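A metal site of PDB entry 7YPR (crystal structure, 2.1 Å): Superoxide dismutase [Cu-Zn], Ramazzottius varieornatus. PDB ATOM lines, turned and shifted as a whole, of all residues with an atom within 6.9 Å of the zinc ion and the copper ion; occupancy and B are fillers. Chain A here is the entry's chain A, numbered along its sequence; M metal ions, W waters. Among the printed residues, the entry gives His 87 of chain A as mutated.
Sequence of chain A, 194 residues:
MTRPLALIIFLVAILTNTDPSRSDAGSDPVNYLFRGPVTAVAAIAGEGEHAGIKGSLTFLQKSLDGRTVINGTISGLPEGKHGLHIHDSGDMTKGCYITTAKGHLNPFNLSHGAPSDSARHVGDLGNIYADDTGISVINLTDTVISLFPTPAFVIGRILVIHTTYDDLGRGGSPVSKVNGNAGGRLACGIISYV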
ATOM      1  N   GLY A  83       6.770  -6.870  14.476  1.00  0.00           N
ATOM      2  CA  GLY A  83       6.755  -7.711  15.657  1.00  0.00           C
ATOM      3  C   GLY A  83       8.017  -7.561  16.490  1.00  0.00           C
ATOM      4  O   GLY A  83       9.128  -7.363  15.965  1.00  0.00           O
ATOM      5  N   LEU A  84       7.847  -7.636  17.802  1.00  0.00           N
ATOM      6  CA  LEU A  84       8.900  -7.452  18.784  1.00  0.00           C
ATOM      7  C   LEU A  84       8.839  -8.651  19.727  1.00  0.00           C
ATOM      8  O   LEU A  84       7.911  -8.770  20.523  1.00  0.00           O
ATOM      9  CB  LEU A  84       8.702  -6.143  19.562  1.00  0.00           C
ATOM     10  CG  LEU A  84       9.680  -5.891  20.695  1.00  0.00           C
ATOM     11  CD1 LEU A  84      11.015  -5.399  20.131  1.00  0.00           C
ATOM     12  CD2 LEU A  84       9.116  -4.890  21.689  1.00  0.00           C
ATOM     13  N   HIS A  85       9.822  -9.547  19.620  1.00  0.00           N
ATOM     14  CA  HIS A  85       9.736 -10.835  20.307  1.00  0.00           C
ATOM     15  C   HIS A  85      11.067 -11.151  20.964  1.00  0.00           C
ATOM     16  O   HIS A  85      12.136 -10.787  20.461  1.00  0.00           O
ATOM     17  CB  HIS A  85       9.373 -11.986  19.329  1.00  0.00           C
ATOM     18  CG  HIS A  85       8.090 -11.780  18.586  1.00  0.00           C
ATOM     19  ND1 HIS A  85       7.911 -12.182  17.285  1.00  0.00           N
ATOM     20  CD2 HIS A  85       6.910 -11.219  18.971  1.00  0.00           C
ATOM     21  CE1 HIS A  85       6.695 -11.870  16.880  1.00  0.00           C
ATOM     22  NE2 HIS A  85       6.062 -11.289  17.887  1.00  0.00           N
ATOM     23  N   ILE A  86      10.994 -11.823  22.102  1.00  0.00           N
ATOM     24  CA  ILE A  86      12.175 -12.376  22.754  1.00  0.00           C
ATOM     25  C   ILE A  86      12.296 -13.844  22.386  1.00  0.00           C
ATOM     26  O   ILE A  86      11.380 -14.643  22.630  1.00  0.00           O
ATOM     27  CB  ILE A  86      12.102 -12.197  24.269  1.00  0.00           C
ATOM     28  CG1 ILE A  86      11.977 -10.695  24.576  1.00  0.00           C
ATOM     29  CG2 ILE A  86      13.337 -12.837  24.942  1.00  0.00           C
ATOM     30  CD1 ILE A  86      11.646 -10.425  26.039  1.00  0.00           C
ATOM     31  N   HIS A  87      13.421 -14.214  21.805  1.00  0.00           N
ATOM     32  CA  HIS A  87      13.647 -15.561  21.305  1.00  0.00           C
ATOM     33  C   HIS A  87      14.172 -16.453  22.424  1.00  0.00           C
ATOM     34  O   HIS A  87      14.720 -15.994  23.424  1.00  0.00           O
ATOM     35  CB  HIS A  87      14.633 -15.512  20.127  1.00  0.00           C
ATOM     36  CG  HIS A  87      14.622 -16.745  19.289  1.00  0.00           C
ATOM     37  ND1 HIS A  87      15.322 -17.885  19.639  1.00  0.00           N
ATOM     38  CD2 HIS A  87      13.985 -17.034  18.125  1.00  0.00           C
ATOM     39  CE1 HIS A  87      15.123 -18.819  18.722  1.00  0.00           C
ATOM     40  NE2 HIS A  87      14.326 -18.327  17.792  1.00  0.00           N
ATOM     41  N   GLY A 103      12.425 -21.185  18.415  1.00  0.00           N
ATOM     42  CA  GLY A 103      11.289 -20.269  18.486  1.00  0.00           C
ATOM     43  C   GLY A 103      11.309 -19.317  19.679  1.00  0.00           C
ATOM     44  O   GLY A 103      12.313 -19.162  20.387  1.00  0.00           O
ATOM     45  N   HIS A 104      10.165 -18.666  19.907  1.00  0.00           N
ATOM     46  CA  HIS A 104      10.071 -17.614  20.925  1.00  0.00           C
ATOM     47  C   HIS A 104      10.262 -18.192  22.324  1.00  0.00           C
ATOM     48  O   HIS A 104       9.949 -19.355  22.583  1.00  0.00           O
ATOM     49  CB  HIS A 104       8.712 -16.901  20.863  1.00  0.00           C
ATOM     50  CG  HIS A 104       8.493 -16.152  19.579  1.00  0.00           C
ATOM     51  ND1 HIS A 104       7.247 -15.793  19.137  1.00  0.00           N
ATOM     52  CD2 HIS A 104       9.365 -15.705  18.653  1.00  0.00           C
ATOM     53  CE1 HIS A 104       7.348 -15.143  17.992  1.00  0.00           C
ATOM     54  NE2 HIS A 104       8.633 -15.075  17.681  1.00  0.00           N
ATOM     55  N   LEU A 105      10.762 -17.339  23.218  1.00  0.00           N
ATOM     56  CA  LEU A 105      10.964 -17.742  24.608  1.00  0.00           C
ATOM     57  C   LEU A 105       9.647 -18.253  25.204  1.00  0.00           C
ATOM     58  O   LEU A 105       8.674 -17.504  25.283  1.00  0.00           O
ATOM     59  CB  LEU A 105      11.491 -16.546  25.409  1.00  0.00           C
ATOM     60  CG  LEU A 105      11.819 -16.781  26.876  1.00  0.00           C
ATOM     61  CD1 LEU A 105      12.915 -17.869  27.034  1.00  0.00           C
ATOM     62  CD2 LEU A 105      12.206 -15.492  27.563  1.00  0.00           C
ATOM     63  N   ASN A 106       9.611 -19.528  25.592  1.00  0.00           N
ATOM     64  CA  ASN A 106       8.316 -20.124  25.911  1.00  0.00           C
ATOM     65  C   ASN A 106       8.417 -21.160  27.037  1.00  0.00           C
ATOM     66  O   ASN A 106       8.062 -22.323  26.836  1.00  0.00           O
ATOM     67  CB  ASN A 106       7.716 -20.737  24.637  1.00  0.00           C
ATOM     68  CG  ASN A 106       6.291 -21.227  24.836  1.00  0.00           C
ATOM     69  OD1 ASN A 106       5.605 -20.816  25.770  1.00  0.00           O
ATOM     70  ND2 ASN A 106       5.847 -22.123  23.963  1.00  0.00           N
ATOM     71  N   SER A 111       0.810 -21.185  23.475  1.00  0.00           N
ATOM     72  CA  SER A 111       0.857 -20.829  22.058  1.00  0.00           C
ATOM     73  C   SER A 111       1.075 -19.316  21.879  1.00  0.00           C
ATOM     74  O   SER A 111       0.932 -18.529  22.805  1.00  0.00           O
ATOM     75  CB  SER A 111      -0.427 -21.270  21.371  1.00  0.00           C
ATOM     76  OG  SER A 111      -1.534 -20.881  22.146  1.00  0.00           O
ATOM     77  N   HIS A 112       1.419 -18.927  20.657  1.00  0.00           N
ATOM     78  CA  HIS A 112       1.724 -17.540  20.387  1.00  0.00           C
ATOM     79  C   HIS A 112       0.484 -16.674  20.583  1.00  0.00           C
ATOM     80  O   HIS A 112      -0.602 -17.017  20.104  1.00  0.00           O
ATOM     81  CB  HIS A 112       2.281 -17.374  18.964  1.00  0.00           C
ATOM     82  CG  HIS A 112       2.561 -15.951  18.591  1.00  0.00           C
ATOM     83  ND1 HIS A 112       3.705 -15.285  18.981  1.00  0.00           N
ATOM     84  CD2 HIS A 112       1.822 -15.044  17.894  1.00  0.00           C
ATOM     85  CE1 HIS A 112       3.674 -14.037  18.534  1.00  0.00           C
ATOM     86  NE2 HIS A 112       2.546 -13.867  17.875  1.00  0.00           N
ATOM     87  N   GLY A 113       0.633 -15.548  21.281  1.00  0.00           N
ATOM     88  CA  GLY A 113      -0.486 -14.650  21.467  1.00  0.00           C
ATOM     89  C   GLY A 113      -0.096 -13.190  21.487  1.00  0.00           C
ATOM     90  O   GLY A 113       1.058 -12.829  21.244  1.00  0.00           O
ATOM     91  N   ARG A 120      -0.044 -16.783  25.680  1.00  0.00           N
ATOM     92  CA  ARG A 120       1.062 -16.153  24.967  1.00  0.00           C
ATOM     93  C   ARG A 120       2.366 -16.805  25.382  1.00  0.00           C
ATOM     94  O   ARG A 120       2.456 -17.452  26.425  1.00  0.00           O
ATOM     95  CB  ARG A 120       1.125 -14.643  25.246  1.00  0.00           C
ATOM     96  CG  ARG A 120       1.112 -14.313  26.738  1.00  0.00           C
ATOM     97  CD  ARG A 120       1.473 -12.859  26.973  1.00  0.00           C
ATOM     98  NE  ARG A 120       2.919 -12.635  26.924  1.00  0.00           N
ATOM     99  CZ  ARG A 120       3.510 -11.526  27.331  1.00  0.00           C
ATOM    100  NH1 ARG A 120       2.813 -10.495  27.787  1.00  0.00           N
ATOM    101  NH2 ARG A 120       4.843 -11.427  27.249  1.00  0.00           N
ATOM    102  N   HIS A 121       3.385 -16.638  24.532  1.00  0.00           N
ATOM    103  CA  HIS A 121       4.734 -16.942  24.969  1.00  0.00           C
ATOM    104  C   HIS A 121       5.235 -15.839  25.887  1.00  0.00           C
ATOM    105  O   HIS A 121       4.806 -14.694  25.793  1.00  0.00           O
ATOM    106  CB  HIS A 121       5.655 -17.046  23.754  1.00  0.00           C
ATOM    107  CG  HIS A 121       5.219 -18.073  22.758  1.00  0.00           C
ATOM    108  ND1 HIS A 121       5.392 -17.898  21.408  1.00  0.00           N
ATOM    109  CD2 HIS A 121       4.652 -19.291  22.916  1.00  0.00           C
ATOM    110  CE1 HIS A 121       4.929 -18.958  20.764  1.00  0.00           C
ATOM    111  NE2 HIS A 121       4.482 -19.820  21.659  1.00  0.00           N
ATOM    112  N   VAL A 122       6.160 -16.181  26.778  1.00  0.00           N
ATOM    113  CA  VAL A 122       6.835 -15.118  27.527  1.00  0.00           C
ATOM    114  C   VAL A 122       7.418 -14.079  26.582  1.00  0.00           C
ATOM    115  O   VAL A 122       7.308 -12.870  26.813  1.00  0.00           O
ATOM    116  CB  VAL A 122       7.917 -15.708  28.451  1.00  0.00           C
ATOM    117  CG1 VAL A 122       8.842 -14.600  28.956  1.00  0.00           C
ATOM    118  CG2 VAL A 122       7.267 -16.417  29.634  1.00  0.00           C
ATOM    119  N   GLY A 123       7.998 -14.529  25.474  1.00  0.00           N
ATOM    120  CA  GLY A 123       8.610 -13.587  24.574  1.00  0.00           C
ATOM    121  C   GLY A 123       7.695 -12.775  23.677  1.00  0.00           C
ATOM    122  O   GLY A 123       8.206 -12.072  22.806  1.00  0.00           O
ATOM    123  N   ASP A 124       6.367 -12.824  23.857  1.00  0.00           N
ATOM    124  CA  ASP A 124       5.432 -12.167  22.936  1.00  0.00           C
ATOM    125  C   ASP A 124       5.173 -10.725  23.416  1.00  0.00           C
ATOM    126  O   ASP A 124       4.318 -10.494  24.265  1.00  0.00           O
ATOM    127  CB  ASP A 124       4.124 -12.932  22.845  1.00  0.00           C
ATOM    128  CG  ASP A 124       4.265 -14.278  22.131  1.00  0.00           C
ATOM    129  OD1 ASP A 124       5.323 -14.542  21.521  1.00  0.00           O
ATOM    130  OD2 ASP A 124       3.301 -15.082  22.184  1.00  0.00           O
ATOM    131  N   LEU A 125       5.883  -9.755  22.824  1.00  0.00           N
ATOM    132  CA  LEU A 125       5.757  -8.359  23.223  1.00  0.00           C
ATOM    133  C   LEU A 125       4.977  -7.525  22.202  1.00  0.00           C
ATOM    134  O   LEU A 125       4.904  -6.305  22.336  1.00  0.00           O
ATOM    135  CB  LEU A 125       7.143  -7.736  23.473  1.00  0.00           C
ATOM    136  CG  LEU A 125       7.960  -8.418  24.584  1.00  0.00           C
ATOM    137  CD1 LEU A 125       9.291  -7.718  24.855  1.00  0.00           C
ATOM    138  CD2 LEU A 125       7.154  -8.481  25.865  1.00  0.00           C
ATOM    139  N   VAL A 160      14.163  -9.623  19.094  1.00  0.00           N
ATOM    140  CA  VAL A 160      14.071  -9.606  17.647  1.00  0.00           C
ATOM    141  C   VAL A 160      13.081  -8.526  17.214  1.00  0.00           C
ATOM    142  O   VAL A 160      12.006  -8.400  17.808  1.00  0.00           O
ATOM    143  CB  VAL A 160      13.595 -10.983  17.107  1.00  0.00           C
ATOM    144  CG1 VAL A 160      13.316 -10.932  15.606  1.00  0.00           C
ATOM    145  CG2 VAL A 160      14.632 -12.051  17.396  1.00  0.00           C
ATOM    146  N   HIS A 162      10.972  -7.842  13.850  1.00  0.00           N
ATOM    147  CA  HIS A 162      10.629  -8.601  12.668  1.00  0.00           C
ATOM    148  C   HIS A 162      10.381  -7.705  11.462  1.00  0.00           C
ATOM    149  O   HIS A 162      10.096  -6.509  11.574  1.00  0.00           O
ATOM    150  CB  HIS A 162       9.393  -9.457  12.919  1.00  0.00           C
ATOM    151  CG  HIS A 162       9.685 -10.760  13.590  1.00  0.00           C
ATOM    152  ND1 HIS A 162      10.249 -11.826  12.935  1.00  0.00           N
ATOM    153  CD2 HIS A 162       9.453 -11.190  14.856  1.00  0.00           C
ATOM    154  CE1 HIS A 162      10.368 -12.852  13.757  1.00  0.00           C
ATOM    155  NE2 HIS A 162       9.897 -12.492  14.940  1.00  0.00           N
ATOM    156  N   ASP A 166       3.280  -8.578  13.743  1.00  0.00           N
ATOM    157  CA  ASP A 166       2.808  -9.743  14.484  1.00  0.00           C
ATOM    158  C   ASP A 166       1.281  -9.768  14.396  1.00  0.00           C
ATOM    159  O   ASP A 166       0.629  -8.778  14.747  1.00  0.00           O
ATOM    160  CB  ASP A 166       3.282  -9.584  15.918  1.00  0.00           C
ATOM    161  CG  ASP A 166       2.885 -10.726  16.831  1.00  0.00           C
ATOM    162  OD1 ASP A 166       2.183 -11.665  16.417  1.00  0.00           O
ATOM    163  OD2 ASP A 166       3.294 -10.663  18.014  1.00  0.00           O
ATOM    164  N   SER A 176       0.524 -18.726  12.486  1.00  0.00           N
ATOM    165  CA  SER A 176      -0.024 -17.639  13.290  1.00  0.00           C
ATOM    166  C   SER A 176       0.113 -17.937  14.779  1.00  0.00           C
ATOM    167  O   SER A 176       0.505 -17.067  15.567  1.00  0.00           O
ATOM    168  CB  SER A 176      -1.500 -17.401  12.928  1.00  0.00           C
ATOM    169  OG  SER A 176      -1.633 -16.649  11.743  1.00  0.00           O
ATOM    170  N   LYS A 177      -0.205 -19.167  15.189  1.00  0.00           N
ATOM    171  CA  LYS A 177      -0.089 -19.546  16.601  1.00  0.00           C
ATOM    172  C   LYS A 177       1.293 -20.033  16.985  1.00  0.00           C
ATOM    173  O   LYS A 177       1.508 -20.424  18.133  1.00  0.00           O
ATOM    174  CB  LYS A 177      -1.130 -20.622  16.952  1.00  0.00           C
ATOM    175  CG  LYS A 177      -2.552 -20.178  16.705  1.00  0.00           C
ATOM    176  CD  LYS A 177      -3.018 -19.312  17.858  1.00  0.00           C
ATOM    177  CE  LYS A 177      -4.485 -19.550  18.198  1.00  0.00           C
ATOM    178  NZ  LYS A 177      -5.035 -18.352  18.901  1.00  0.00           N
ATOM    179  N   VAL A 178       2.246 -20.027  16.048  1.00  0.00           N
ATOM    180  CA  VAL A 178       3.636 -20.328  16.360  1.00  0.00           C
ATOM    181  C   VAL A 178       4.433 -19.051  16.626  1.00  0.00           C
ATOM    182  O   VAL A 178       5.165 -18.969  17.615  1.00  0.00           O
ATOM    183  CB  VAL A 178       4.248 -21.150  15.210  1.00  0.00           C
ATOM    184  CG1 VAL A 178       5.741 -21.362  15.430  1.00  0.00           C
ATOM    185  CG2 VAL A 178       3.533 -22.485  15.114  1.00  0.00           C
ATOM    186  N   ASN A 179       4.242 -18.036  15.804  1.00  0.00           N
ATOM    187  CA  ASN A 179       5.013 -16.817  15.973  1.00  0.00           C
ATOM    188  C   ASN A 179       4.318 -15.572  15.423  1.00  0.00           C
ATOM    189  O   ASN A 179       4.995 -14.545  15.271  1.00  0.00           O
ATOM    190  CB  ASN A 179       6.386 -16.954  15.290  1.00  0.00           C
ATOM    191  CG  ASN A 179       6.269 -17.439  13.869  1.00  0.00           C
ATOM    192  OD1 ASN A 179       5.417 -16.965  13.095  1.00  0.00           O
ATOM    193  ND2 ASN A 179       7.143 -18.358  13.494  1.00  0.00           N
ATOM    194  N   GLY A 180       3.033 -15.619  15.112  1.00  0.00           N
ATOM    195  CA  GLY A 180       2.367 -14.434  14.603  1.00  0.00           C
ATOM    196  C   GLY A 180       2.667 -14.095  13.164  1.00  0.00           C
ATOM    197  O   GLY A 180       2.222 -13.052  12.687  1.00  0.00           O
ATOM    198  N   ALA A 182       5.203 -12.994  11.489  1.00  0.00           N
ATOM    199  CA  ALA A 182       5.764 -11.667  11.300  1.00  0.00           C
ATOM    200  C   ALA A 182       6.952 -11.659  10.356  1.00  0.00           C
ATOM    201  O   ALA A 182       7.572 -10.612  10.182  1.00  0.00           O
ATOM    202  CB  ALA A 182       6.143 -11.067  12.643  1.00  0.00           C
ATOM    203  N   GLY A 183       7.286 -12.799   9.736  1.00  0.00           N
ATOM    204  CA  GLY A 183       8.332 -12.811   8.720  1.00  0.00           C
ATOM    205  C   GLY A 183       9.733 -12.919   9.267  1.00  0.00           C
ATOM    206  O   GLY A 183       9.947 -13.478  10.344  1.00  0.00           O
ATOM    207  N   ARG A 185      13.782 -11.448  10.240  1.00  0.00           N
ATOM    208  CA  ARG A 185      14.340 -10.555  11.237  1.00  0.00           C
ATOM    209  C   ARG A 185      14.995  -9.379  10.529  1.00  0.00           C
ATOM    210  O   ARG A 185      15.716  -9.565   9.549  1.00  0.00           O
ATOM    211  CB  ARG A 185      15.339 -11.276  12.130  1.00  0.00           C
ATOM    212  CG  ARG A 185      14.803 -12.598  12.668  1.00  0.00           C
ATOM    213  CD  ARG A 185      15.897 -13.416  13.331  1.00  0.00           C
ATOM    214  NE  ARG A 185      15.545 -14.824  13.331  1.00  0.00           N
ATOM    215  CZ  ARG A 185      16.039 -15.730  12.502  1.00  0.00           C
ATOM    216  NH1 ARG A 185      16.957 -15.419  11.605  1.00  0.00           N
ATOM    217  NH2 ARG A 185      15.595 -16.980  12.577  1.00  0.00           N
HETATM  218 ZN    ZN M   1       5.369 -15.997  20.309  1.00  0.00          ZN
HETATM  219 CU    CU M   2       9.170 -13.627  16.474  1.00  0.00          CU
HETATM  220  O   HOH W   1      11.787 -14.882  16.543  1.00  0.00           O
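The side-chain carboxylate (OD2) of Asp 124 lies within hydrogen-bond range of the backbone NH (N) of Gly 113 (2.9 Å).
O of Asp 124 sits at hydrogen-bond distance from NH2 of Arg 120, at 3.2 Å.
The backbone carbonyl oxygen (O) of Gly 83 sits at hydrogen-bond distance from the backbone NH (N) of His 162 (2.8 Å).
The backbone carbonyl oxygen of Gly 183 is in hydrogen-bond range of a ring nitrogen (ND1) of His 162.
The backbone NH (N) of Val 160 sits at hydrogen-bond distance from the backbone carbonyl oxygen (O) of His 85.
NE2 of His 112 lies close to N of Gly 180.
NE2 of His 112 sits at hydrogen-bond distance from OD1 of Asp 166, 2.7 Å away.
The backbone carbonyl oxygen (O) of Lys 177 is in hydrogen-bond range of the backbone NH (N) of His 112 (2.9 Å).
Of the 29 residues printed, 4 come within 4 Å of the zinc ion.
Along chain A the residues within 4 Å of the zinc ion span positions 104 to 124.
The zinc ion is bound by OD1 of Asp 124, ND1 of His 121, ND1 of His 104 and ND1 of His 112.
The zinc ion has four donor atoms within binding distance.
The copper ion is bound by a ring nitrogen (NE2) of His 104, a ring nitrogen (NE2) of His 162 and a ring nitrogen (ND1) of His 85.
The copper ion has three donor atoms within binding distance.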
